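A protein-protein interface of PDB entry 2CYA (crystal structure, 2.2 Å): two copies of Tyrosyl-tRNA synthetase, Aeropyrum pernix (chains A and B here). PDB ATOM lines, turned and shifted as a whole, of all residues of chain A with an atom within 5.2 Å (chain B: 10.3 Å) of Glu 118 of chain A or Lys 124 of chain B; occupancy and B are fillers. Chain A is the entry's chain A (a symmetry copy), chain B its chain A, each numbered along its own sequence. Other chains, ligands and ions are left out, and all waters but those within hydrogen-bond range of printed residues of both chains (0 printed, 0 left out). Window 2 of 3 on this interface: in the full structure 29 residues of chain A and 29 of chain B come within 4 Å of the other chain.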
ATOM      1  N   THR A  75      23.242  33.694 -29.621  1.00  0.00           N
ATOM      2  CA  THR A  75      24.296  33.266 -28.720  1.00  0.00           C
ATOM      3  C   THR A  75      24.198  31.817 -28.276  1.00  0.00           C
ATOM      4  O   THR A  75      25.219  31.135 -28.197  1.00  0.00           O
ATOM      5  CB  THR A  75      24.360  34.169 -27.472  1.00  0.00           C
ATOM      6  OG1 THR A  75      23.142  34.049 -26.731  1.00  0.00           O
ATOM      7  CG2 THR A  75      24.572  35.644 -27.887  1.00  0.00           C
ATOM      8  N   TRP A  76      22.986  31.340 -27.999  1.00  0.00           N
ATOM      9  CA  TRP A  76      22.822  29.956 -27.574  1.00  0.00           C
ATOM     10  C   TRP A  76      23.157  29.004 -28.726  1.00  0.00           C
ATOM     11  O   TRP A  76      23.711  27.925 -28.522  1.00  0.00           O
ATOM     12  CB  TRP A  76      21.393  29.726 -27.045  1.00  0.00           C
ATOM     13  CG  TRP A  76      21.222  30.259 -25.645  1.00  0.00           C
ATOM     14  CD1 TRP A  76      21.703  31.439 -25.150  1.00  0.00           C
ATOM     15  CD2 TRP A  76      20.531  29.623 -24.559  1.00  0.00           C
ATOM     16  NE1 TRP A  76      21.353  31.580 -23.825  1.00  0.00           N
ATOM     17  CE2 TRP A  76      20.638  30.476 -23.438  1.00  0.00           C
ATOM     18  CE3 TRP A  76      19.834  28.415 -24.425  1.00  0.00           C
ATOM     19  CZ2 TRP A  76      20.076  30.157 -22.199  1.00  0.00           C
ATOM     20  CZ3 TRP A  76      19.269  28.097 -23.187  1.00  0.00           C
ATOM     21  CH2 TRP A  76      19.395  28.966 -22.096  1.00  0.00           C
ATOM     22  N   MET A  88      30.560  32.174 -23.349  1.00  0.00           N
ATOM     23  CA  MET A  88      29.476  33.116 -23.574  1.00  0.00           C
ATOM     24  C   MET A  88      29.865  34.594 -23.546  1.00  0.00           C
ATOM     25  O   MET A  88      29.223  35.413 -24.218  1.00  0.00           O
ATOM     26  CB  MET A  88      28.337  32.846 -22.579  1.00  0.00           C
ATOM     27  CG  MET A  88      27.622  31.503 -22.802  1.00  0.00           C
ATOM     28  SD  MET A  88      26.950  31.311 -24.500  1.00  0.00           S
ATOM     29  CE  MET A  88      25.549  32.413 -24.396  1.00  0.00           C
ATOM     30  N   ARG A  92      29.261  37.147 -26.661  1.00  0.00           N
ATOM     31  CA  ARG A  92      28.551  38.408 -26.486  1.00  0.00           C
ATOM     32  C   ARG A  92      29.405  39.543 -27.026  1.00  0.00           C
ATOM     33  O   ARG A  92      28.893  40.482 -27.633  1.00  0.00           O
ATOM     34  CB  ARG A  92      28.272  38.677 -25.004  1.00  0.00           C
ATOM     35  CG  ARG A  92      26.795  38.920 -24.680  1.00  0.00           C
ATOM     36  CD  ARG A  92      26.188  37.744 -23.930  1.00  0.00           C
ATOM     37  NE  ARG A  92      26.973  37.437 -22.730  1.00  0.00           N
ATOM     38  CZ  ARG A  92      26.721  36.431 -21.893  1.00  0.00           C
ATOM     39  NH1 ARG A  92      25.690  35.617 -22.115  1.00  0.00           N
ATOM     40  NH2 ARG A  92      27.511  36.241 -20.838  1.00  0.00           N
ATOM     41  N   ASP A 116      19.203  39.546 -27.954  1.00  0.00           N
ATOM     42  CA  ASP A 116      20.120  38.478 -27.531  1.00  0.00           C
ATOM     43  C   ASP A 116      19.240  37.228 -27.333  1.00  0.00           C
ATOM     44  O   ASP A 116      18.168  37.312 -26.743  1.00  0.00           O
ATOM     45  CB  ASP A 116      20.792  38.852 -26.195  1.00  0.00           C
ATOM     46  CG  ASP A 116      21.830  37.827 -25.750  1.00  0.00           C
ATOM     47  OD1 ASP A 116      21.502  36.621 -25.666  1.00  0.00           O
ATOM     48  OD2 ASP A 116      22.979  38.225 -25.488  1.00  0.00           O
ATOM     49  N   ALA A 117      19.669  36.076 -27.837  1.00  0.00           N
ATOM     50  CA  ALA A 117      18.880  34.850 -27.683  1.00  0.00           C
ATOM     51  C   ALA A 117      18.457  34.613 -26.220  1.00  0.00           C
ATOM     52  O   ALA A 117      17.459  33.944 -25.952  1.00  0.00           O
ATOM     53  CB  ALA A 117      19.683  33.663 -28.190  1.00  0.00           C
ATOM     54  N   GLU A 118      19.220  35.163 -25.279  1.00  0.00           N
ATOM     55  CA  GLU A 118      18.915  35.000 -23.862  1.00  0.00           C
ATOM     56  C   GLU A 118      17.518  35.489 -23.501  1.00  0.00           C
ATOM     57  O   GLU A 118      16.881  34.937 -22.601  1.00  0.00           O
ATOM     58  CB  GLU A 118      19.931  35.754 -23.002  1.00  0.00           C
ATOM     59  CG  GLU A 118      19.903  35.343 -21.549  1.00  0.00           C
ATOM     60  CD  GLU A 118      21.195  34.684 -21.111  1.00  0.00           C
ATOM     61  OE1 GLU A 118      21.735  33.818 -21.850  1.00  0.00           O
ATOM     62  OE2 GLU A 118      21.671  35.034 -20.013  1.00  0.00           O
ATOM     63  N   GLU A 119      17.045  36.523 -24.186  1.00  0.00           N
ATOM     64  CA  GLU A 119      15.720  37.055 -23.915  1.00  0.00           C
ATOM     65  C   GLU A 119      14.672  36.032 -24.321  1.00  0.00           C
ATOM     66  O   GLU A 119      13.636  35.917 -23.684  1.00  0.00           O
ATOM     67  CB  GLU A 119      15.478  38.369 -24.670  1.00  0.00           C
ATOM     68  CG  GLU A 119      16.564  39.413 -24.458  1.00  0.00           C
ATOM     69  CD  GLU A 119      16.309  40.704 -25.239  1.00  0.00           C
ATOM     70  OE1 GLU A 119      17.306  41.402 -25.560  1.00  0.00           O
ATOM     71  OE2 GLU A 119      15.122  41.014 -25.521  1.00  0.00           O
ATOM     72  N   LEU A 120      14.929  35.288 -25.389  1.00  0.00           N
ATOM     73  CA  LEU A 120      13.972  34.277 -25.803  1.00  0.00           C
ATOM     74  C   LEU A 120      14.068  33.075 -24.855  1.00  0.00           C
ATOM     75  O   LEU A 120      13.054  32.509 -24.451  1.00  0.00           O
ATOM     76  CB  LEU A 120      14.258  33.835 -27.245  1.00  0.00           C
ATOM     77  CG  LEU A 120      13.582  34.627 -28.381  1.00  0.00           C
ATOM     78  CD1 LEU A 120      13.847  36.121 -28.238  1.00  0.00           C
ATOM     79  CD2 LEU A 120      14.099  34.124 -29.707  1.00  0.00           C
ATOM     80  N   ALA A 121      15.295  32.711 -24.496  1.00  0.00           N
ATOM     81  CA  ALA A 121      15.557  31.578 -23.624  1.00  0.00           C
ATOM     82  C   ALA A 121      14.889  31.684 -22.257  1.00  0.00           C
ATOM     83  O   ALA A 121      14.615  30.660 -21.627  1.00  0.00           O
ATOM     84  CB  ALA A 121      17.083  31.389 -23.445  1.00  0.00           C
ATOM     85  N   SER A 122      14.622  32.918 -21.827  1.00  0.00           N
ATOM     86  CA  SER A 122      14.015  33.218 -20.533  1.00  0.00           C
ATOM     87  C   SER A 122      12.513  33.132 -20.546  1.00  0.00           C
ATOM     88  O   SER A 122      11.878  33.350 -19.522  1.00  0.00           O
ATOM     89  CB  SER A 122      14.359  34.646 -20.084  1.00  0.00           C
ATOM     90  OG  SER A 122      15.751  34.852 -20.003  1.00  0.00           O
ATOM     91  N   ALA B 117       6.112  21.090 -13.523  1.00  0.00           N
ATOM     92  CA  ALA B 117       7.197  21.269 -14.492  1.00  0.00           C
ATOM     93  C   ALA B 117       7.277  22.719 -15.012  1.00  0.00           C
ATOM     94  O   ALA B 117       8.335  23.177 -15.444  1.00  0.00           O
ATOM     95  CB  ALA B 117       7.003  20.311 -15.656  1.00  0.00           C
ATOM     96  N   GLU B 118       6.155  23.433 -14.968  1.00  0.00           N
ATOM     97  CA  GLU B 118       6.115  24.813 -15.438  1.00  0.00           C
ATOM     98  C   GLU B 118       7.120  25.707 -14.722  1.00  0.00           C
ATOM     99  O   GLU B 118       7.646  26.650 -15.318  1.00  0.00           O
ATOM    100  CB  GLU B 118       4.718  25.407 -15.250  1.00  0.00           C
ATOM    101  CG  GLU B 118       4.501  26.681 -16.030  1.00  0.00           C
ATOM    102  CD  GLU B 118       3.439  26.528 -17.100  1.00  0.00           C
ATOM    103  OE1 GLU B 118       3.435  25.503 -17.832  1.00  0.00           O
ATOM    104  OE2 GLU B 118       2.603  27.447 -17.210  1.00  0.00           O
ATOM    105  N   GLU B 119       7.379  25.427 -13.451  1.00  0.00           N
ATOM    106  CA  GLU B 119       8.329  26.222 -12.689  1.00  0.00           C
ATOM    107  C   GLU B 119       9.727  26.008 -13.245  1.00  0.00           C
ATOM    108  O   GLU B 119      10.536  26.923 -13.259  1.00  0.00           O
ATOM    109  CB  GLU B 119       8.304  25.850 -11.200  1.00  0.00           C
ATOM    110  CG  GLU B 119       6.915  25.874 -10.581  1.00  0.00           C
ATOM    111  CD  GLU B 119       6.915  25.479  -9.102  1.00  0.00           C
ATOM    112  OE1 GLU B 119       5.863  24.978  -8.628  1.00  0.00           O
ATOM    113  OE2 GLU B 119       7.959  25.676  -8.425  1.00  0.00           O
ATOM    114  N   LEU B 120      10.024  24.798 -13.699  1.00  0.00           N
ATOM    115  CA  LEU B 120      11.339  24.548 -14.265  1.00  0.00           C
ATOM    116  C   LEU B 120      11.407  25.168 -15.667  1.00  0.00           C
ATOM    117  O   LEU B 120      12.409  25.777 -16.038  1.00  0.00           O
ATOM    118  CB  LEU B 120      11.605  23.039 -14.342  1.00  0.00           C
ATOM    119  CG  LEU B 120      12.248  22.365 -13.114  1.00  0.00           C
ATOM    120  CD1 LEU B 120      11.468  22.686 -11.846  1.00  0.00           C
ATOM    121  CD2 LEU B 120      12.296  20.873 -13.342  1.00  0.00           C
ATOM    122  N   ALA B 121      10.326  25.020 -16.425  1.00  0.00           N
ATOM    123  CA  ALA B 121      10.241  25.526 -17.785  1.00  0.00           C
ATOM    124  C   ALA B 121      10.453  27.032 -17.896  1.00  0.00           C
ATOM    125  O   ALA B 121      10.879  27.515 -18.947  1.00  0.00           O
ATOM    126  CB  ALA B 121       8.878  25.143 -18.409  1.00  0.00           C
ATOM    127  N   SER B 122      10.167  27.748 -16.809  1.00  0.00           N
ATOM    128  CA  SER B 122      10.276  29.203 -16.736  1.00  0.00           C
ATOM    129  C   SER B 122      11.667  29.680 -16.420  1.00  0.00           C
ATOM    130  O   SER B 122      11.901  30.879 -16.340  1.00  0.00           O
ATOM    131  CB  SER B 122       9.368  29.767 -15.635  1.00  0.00           C
ATOM    132  OG  SER B 122       8.017  29.413 -15.832  1.00  0.00           O
ATOM    133  N   ASP B 123      12.587  28.761 -16.192  1.00  0.00           N
ATOM    134  CA  ASP B 123      13.931  29.173 -15.841  1.00  0.00           C
ATOM    135  C   ASP B 123      14.870  28.877 -16.987  1.00  0.00           C
ATOM    136  O   ASP B 123      14.997  27.728 -17.413  1.00  0.00           O
ATOM    137  CB  ASP B 123      14.396  28.445 -14.576  1.00  0.00           C
ATOM    138  CG  ASP B 123      15.700  28.997 -14.030  1.00  0.00           C
ATOM    139  OD1 ASP B 123      16.380  29.778 -14.736  1.00  0.00           O
ATOM    140  OD2 ASP B 123      16.053  28.651 -12.885  1.00  0.00           O
ATOM    141  N   LYS B 124      15.525  29.920 -17.480  1.00  0.00           N
ATOM    142  CA  LYS B 124      16.466  29.761 -18.580  1.00  0.00           C
ATOM    143  C   LYS B 124      17.568  28.777 -18.213  1.00  0.00           C
ATOM    144  O   LYS B 124      18.048  28.016 -19.061  1.00  0.00           O
ATOM    145  CB  LYS B 124      17.067  31.118 -18.966  1.00  0.00           C
ATOM    146  CG  LYS B 124      18.027  31.743 -17.964  1.00  0.00           C
ATOM    147  CD  LYS B 124      18.449  33.138 -18.462  1.00  0.00           C
ATOM    148  CE  LYS B 124      19.778  33.596 -17.867  1.00  0.00           C
ATOM    149  NZ  LYS B 124      19.700  33.661 -16.383  1.00  0.00           N
ATOM    150  N   ASP B 125      17.966  28.767 -16.946  1.00  0.00           N
ATOM    151  CA  ASP B 125      19.014  27.842 -16.527  1.00  0.00           C
ATOM    152  C   ASP B 125      18.605  26.392 -16.719  1.00  0.00           C
ATOM    153  O   ASP B 125      19.447  25.542 -16.967  1.00  0.00           O
ATOM    154  CB  ASP B 125      19.405  28.090 -15.073  1.00  0.00           C
ATOM    155  CG  ASP B 125      20.141  29.406 -14.897  1.00  0.00           C
ATOM    156  OD1 ASP B 125      20.735  29.878 -15.894  1.00  0.00           O
ATOM    157  OD2 ASP B 125      20.133  29.959 -13.776  1.00  0.00           O
ATOM    158  N   TYR B 126      17.311  26.107 -16.611  1.00  0.00           N
ATOM    159  CA  TYR B 126      16.865  24.750 -16.822  1.00  0.00           C
ATOM    160  C   TYR B 126      17.120  24.369 -18.286  1.00  0.00           C
ATOM    161  O   TYR B 126      17.698  23.307 -18.565  1.00  0.00           O
ATOM    162  CB  TYR B 126      15.380  24.610 -16.511  1.00  0.00           C
ATOM    163  CG  TYR B 126      14.818  23.285 -16.940  1.00  0.00           C
ATOM    164  CD1 TYR B 126      15.081  22.115 -16.212  1.00  0.00           C
ATOM    165  CD2 TYR B 126      13.991  23.199 -18.054  1.00  0.00           C
ATOM    166  CE1 TYR B 126      14.514  20.900 -16.589  1.00  0.00           C
ATOM    167  CE2 TYR B 126      13.430  21.998 -18.445  1.00  0.00           C
ATOM    168  CZ  TYR B 126      13.687  20.849 -17.717  1.00  0.00           C
ATOM    169  OH  TYR B 126      13.117  19.655 -18.130  1.00  0.00           O
ATOM    170  N   TRP B 127      16.695  25.231 -19.216  1.00  0.00           N
ATOM    171  CA  TRP B 127      16.903  24.943 -20.639  1.00  0.00           C
ATOM    172  C   TRP B 127      18.386  24.961 -20.926  1.00  0.00           C
ATOM    173  O   TRP B 127      18.870  24.227 -21.771  1.00  0.00           O
ATOM    174  CB  TRP B 127      16.116  25.939 -21.517  1.00  0.00           C
ATOM    175  CG  TRP B 127      14.635  25.762 -21.293  1.00  0.00           C
ATOM    176  CD1 TRP B 127      13.809  26.572 -20.547  1.00  0.00           C
ATOM    177  CD2 TRP B 127      13.849  24.624 -21.664  1.00  0.00           C
ATOM    178  NE1 TRP B 127      12.564  25.994 -20.424  1.00  0.00           N
ATOM    179  CE2 TRP B 127      12.563  24.798 -21.099  1.00  0.00           C
ATOM    180  CE3 TRP B 127      14.109  23.464 -22.415  1.00  0.00           C
ATOM    181  CZ2 TRP B 127      11.535  23.854 -21.261  1.00  0.00           C
ATOM    182  CZ3 TRP B 127      13.085  22.526 -22.576  1.00  0.00           C
ATOM    183  CH2 TRP B 127      11.814  22.729 -21.997  1.00  0.00           C
ATOM    184  N   GLY B 128      19.120  25.777 -20.182  1.00  0.00           N
ATOM    185  CA  GLY B 128      20.563  25.795 -20.354  1.00  0.00           C
ATOM    186  C   GLY B 128      21.119  24.393 -20.099  1.00  0.00           C
ATOM    187  O   GLY B 128      22.052  23.945 -20.802  1.00  0.00           O
ATOM    188  N   LEU B 129      20.546  23.693 -19.107  1.00  0.00           N
ATOM    189  CA  LEU B 129      20.967  22.319 -18.756  1.00  0.00           C
ATOM    190  C   LEU B 129      20.489  21.341 -19.808  1.00  0.00           C
ATOM    191  O   LEU B 129      21.184  20.382 -20.146  1.00  0.00           O
ATOM    192  CB  LEU B 129      20.384  21.868 -17.396  1.00  0.00           C
ATOM    193  CG  LEU B 129      21.196  21.987 -16.103  1.00  0.00           C
ATOM    194  CD1 LEU B 129      20.320  21.592 -14.903  1.00  0.00           C
ATOM    195  CD2 LEU B 129      22.415  21.074 -16.176  1.00  0.00           C
ATOM    196  N   VAL B 130      19.277  21.535 -20.307  1.00  0.00           N
ATOM    197  CA  VAL B 130      18.801  20.637 -21.343  1.00  0.00           C
ATOM    198  C   VAL B 130      19.790  20.664 -22.520  1.00  0.00           C
ATOM    199  O   VAL B 130      20.059  19.635 -23.149  1.00  0.00           O
ATOM    200  CB  VAL B 130      17.400  21.038 -21.819  1.00  0.00           C
ATOM    201  CG1 VAL B 130      17.063  20.316 -23.100  1.00  0.00           C
ATOM    202  CG2 VAL B 130      16.378  20.685 -20.730  1.00  0.00           C
ATOM    203  N   ILE B 131      20.347  21.835 -22.805  1.00  0.00           N
ATOM    204  CA  ILE B 131      21.307  21.936 -23.901  1.00  0.00           C
ATOM    205  C   ILE B 131      22.660  21.309 -23.556  1.00  0.00           C
ATOM    206  O   ILE B 131      23.241  20.574 -24.358  1.00  0.00           O
ATOM    207  CB  ILE B 131      21.515  23.398 -24.321  1.00  0.00           C
ATOM    208  CG1 ILE B 131      20.225  23.920 -24.962  1.00  0.00           C
ATOM    209  CG2 ILE B 131      22.665  23.496 -25.313  1.00  0.00           C
ATOM    210  CD1 ILE B 131      20.317  25.344 -25.404  1.00  0.00           C
ATOM    211  N   ARG B 132      23.169  21.594 -22.368  1.00  0.00           N
ATOM    212  CA  ARG B 132      24.440  21.008 -21.980  1.00  0.00           C
ATOM    213  C   ARG B 132      24.331  19.480 -21.950  1.00  0.00           C
ATOM    214  O   ARG B 132      25.265  18.763 -22.346  1.00  0.00           O
ATOM    215  CB  ARG B 132      24.869  21.588 -20.641  1.00  0.00           C
ATOM    216  CG  ARG B 132      25.342  23.035 -20.794  1.00  0.00           C
ATOM    217  CD  ARG B 132      25.379  23.749 -19.481  1.00  0.00           C
ATOM    218  NE  ARG B 132      25.937  22.887 -18.455  1.00  0.00           N
ATOM    219  CZ  ARG B 132      25.673  23.019 -17.161  1.00  0.00           C
ATOM    220  NH1 ARG B 132      24.857  23.992 -16.749  1.00  0.00           N
ATOM    221  NH2 ARG B 132      26.201  22.166 -16.287  1.00  0.00           N
ATOM    222  N   SER B 171      17.537  16.453 -17.201  1.00  0.00           N
ATOM    223  CA  SER B 171      17.745  17.810 -16.734  1.00  0.00           C
ATOM    224  C   SER B 171      16.932  18.131 -15.491  1.00  0.00           C
ATOM    225  O   SER B 171      17.349  18.956 -14.688  1.00  0.00           O
ATOM    226  CB  SER B 171      17.428  18.817 -17.848  1.00  0.00           C
ATOM    227  OG  SER B 171      18.301  18.617 -18.944  1.00  0.00           O
ATOM    228  N   TYR B 175      18.745  19.673 -12.463  1.00  0.00           N
ATOM    229  CA  TYR B 175      18.262  20.985 -12.048  1.00  0.00           C
ATOM    230  C   TYR B 175      17.832  20.983 -10.578  1.00  0.00           C
ATOM    231  O   TYR B 175      18.104  21.937  -9.851  1.00  0.00           O
ATOM    232  CB  TYR B 175      17.082  21.419 -12.915  1.00  0.00           C
ATOM    233  CG  TYR B 175      16.565  22.803 -12.588  1.00  0.00           C
ATOM    234  CD1 TYR B 175      17.155  23.944 -13.145  1.00  0.00           C
ATOM    235  CD2 TYR B 175      15.467  22.974 -11.739  1.00  0.00           C
ATOM    236  CE1 TYR B 175      16.651  25.229 -12.864  1.00  0.00           C
ATOM    237  CE2 TYR B 175      14.963  24.244 -11.452  1.00  0.00           C
ATOM    238  CZ  TYR B 175      15.559  25.365 -12.018  1.00  0.00           C
ATOM    239  OH  TYR B 175      15.062  26.618 -11.722  1.00  0.00           O
ATOM    240  N   ARG B 203      27.684  17.358 -12.609  1.00  0.00           N
ATOM    241  CA  ARG B 203      26.450  17.228 -11.838  1.00  0.00           C
ATOM    242  C   ARG B 203      26.484  15.933 -11.036  1.00  0.00           C
ATOM    243  O   ARG B 203      27.165  14.994 -11.418  1.00  0.00           O
ATOM    244  CB  ARG B 203      25.240  17.203 -12.782  1.00  0.00           C
ATOM    245  CG  ARG B 203      24.934  18.549 -13.398  1.00  0.00           C
ATOM    246  CD  ARG B 203      24.395  19.457 -12.315  1.00  0.00           C
ATOM    247  NE  ARG B 203      24.349  20.837 -12.756  1.00  0.00           N
ATOM    248  CZ  ARG B 203      23.608  21.773 -12.181  1.00  0.00           C
ATOM    249  NH1 ARG B 203      22.842  21.471 -11.135  1.00  0.00           N
ATOM    250  NH2 ARG B 203      23.634  23.010 -12.659  1.00  0.00           N
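The backbone carbonyl oxygen of Glu 118 of chain A sits at hydrogen-bond distance from the side-chain hydroxyl of Ser 122 of chain A, 2.8 Å away. The side-chain amino group (NZ) of Lys 124 of chain B is in salt-bridge range of the side-chain carboxylate (OD1) of Asp 125 of chain B, 3.95 Å away. The side-chain carboxylate (OD1) of Asp 116 of chain A is in hydrogen-bond range of the backbone NH (N) of Glu 118 of chain A (2.7 Å). The side-chain carboxylate (OE1) of Glu 118 of chain A lies within hydrogen-bond range of the indole nitrogen (NE1) of Trp 76 of chain A (3.0 Å). The indole nitrogen (NE1) of Trp 127 of chain B sits at hydrogen-bond distance from the backbone carbonyl oxygen (O) of Ala 121 of chain B (2.7 Å).
Trp 76 of chain A touches Lys 124 of chain B (CH2 to O, 3.5 Å). C of Trp 127 of chain B touches CZ3 of Trp 76 of chain A (3.97 Å). N of Gly 128 of chain B touches CH2 of Trp 76 of chain A, at 3.7 Å. Trp 76 of chain A touches Ile 131 of chain B. Glu 118 of chain A touches Lys 124 of chain B (OE2 to CE, 3.2 Å). O of Ala 121 of chain A touches CB of Lys 124 of chain B, 3.6 Å away. OG of Ser 122 of chain A touches CD of Lys 124 of chain B, 3.5 Å away.
Glu 118 of chain A touches just one residue of chain B: Lys 124. Of chain A, only Trp 76, Glu 118, Ala 121 and Ser 122 come within 4 Å of Lys 124 of chain B. Of chain B, only Lys 124 comes within 4 Å of Ala 121 of chain A. Printed residues of chain A within 4 Å of Ile 131 of chain B: Trp 76. Of the printed residues of chain A, Trp 127 of chain B touches Trp 76. Of the printed residues of chain B, Trp 76 of chain A touches Lys 124 (3.5 Å), Trp 127 (3.97 Å), Gly 128 (3.7 Å) and Ile 131 (3.3 Å). Printed residues of chain A within 4 Å of Gly 128 of chain B: Trp 76 (3.7 Å). The nearest printed residue of chain A that does not touch Lys 124 of chain B is Glu 119 of chain A (6.8 Å). The nearest printed residue of chain A that does not touch Gly 128 of chain B is Ala 121 of chain A (6.8 Å).
Printed residues of chain B that touch a printed residue of chain A: Lys 124, Trp 127, Gly 128 and Ile 131. Hydrophobic or aromatic side chains of chain B that line the printed part of chain A: Ile 131. Along chain B the printed residues that touch a printed residue of chain A span positions 124 to 131. Among the printed residues, 7 pairs touch across the chains. Among the printed residues, no Asp or Glu carboxylate lies within 4 Å of a Lys or Arg side-chain nitrogen of the other chain.
6 positions are printed for both chains. Of the 7 pairs that touch across the chains among the printed residues, none has its exchanged pair printed and touching as well.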
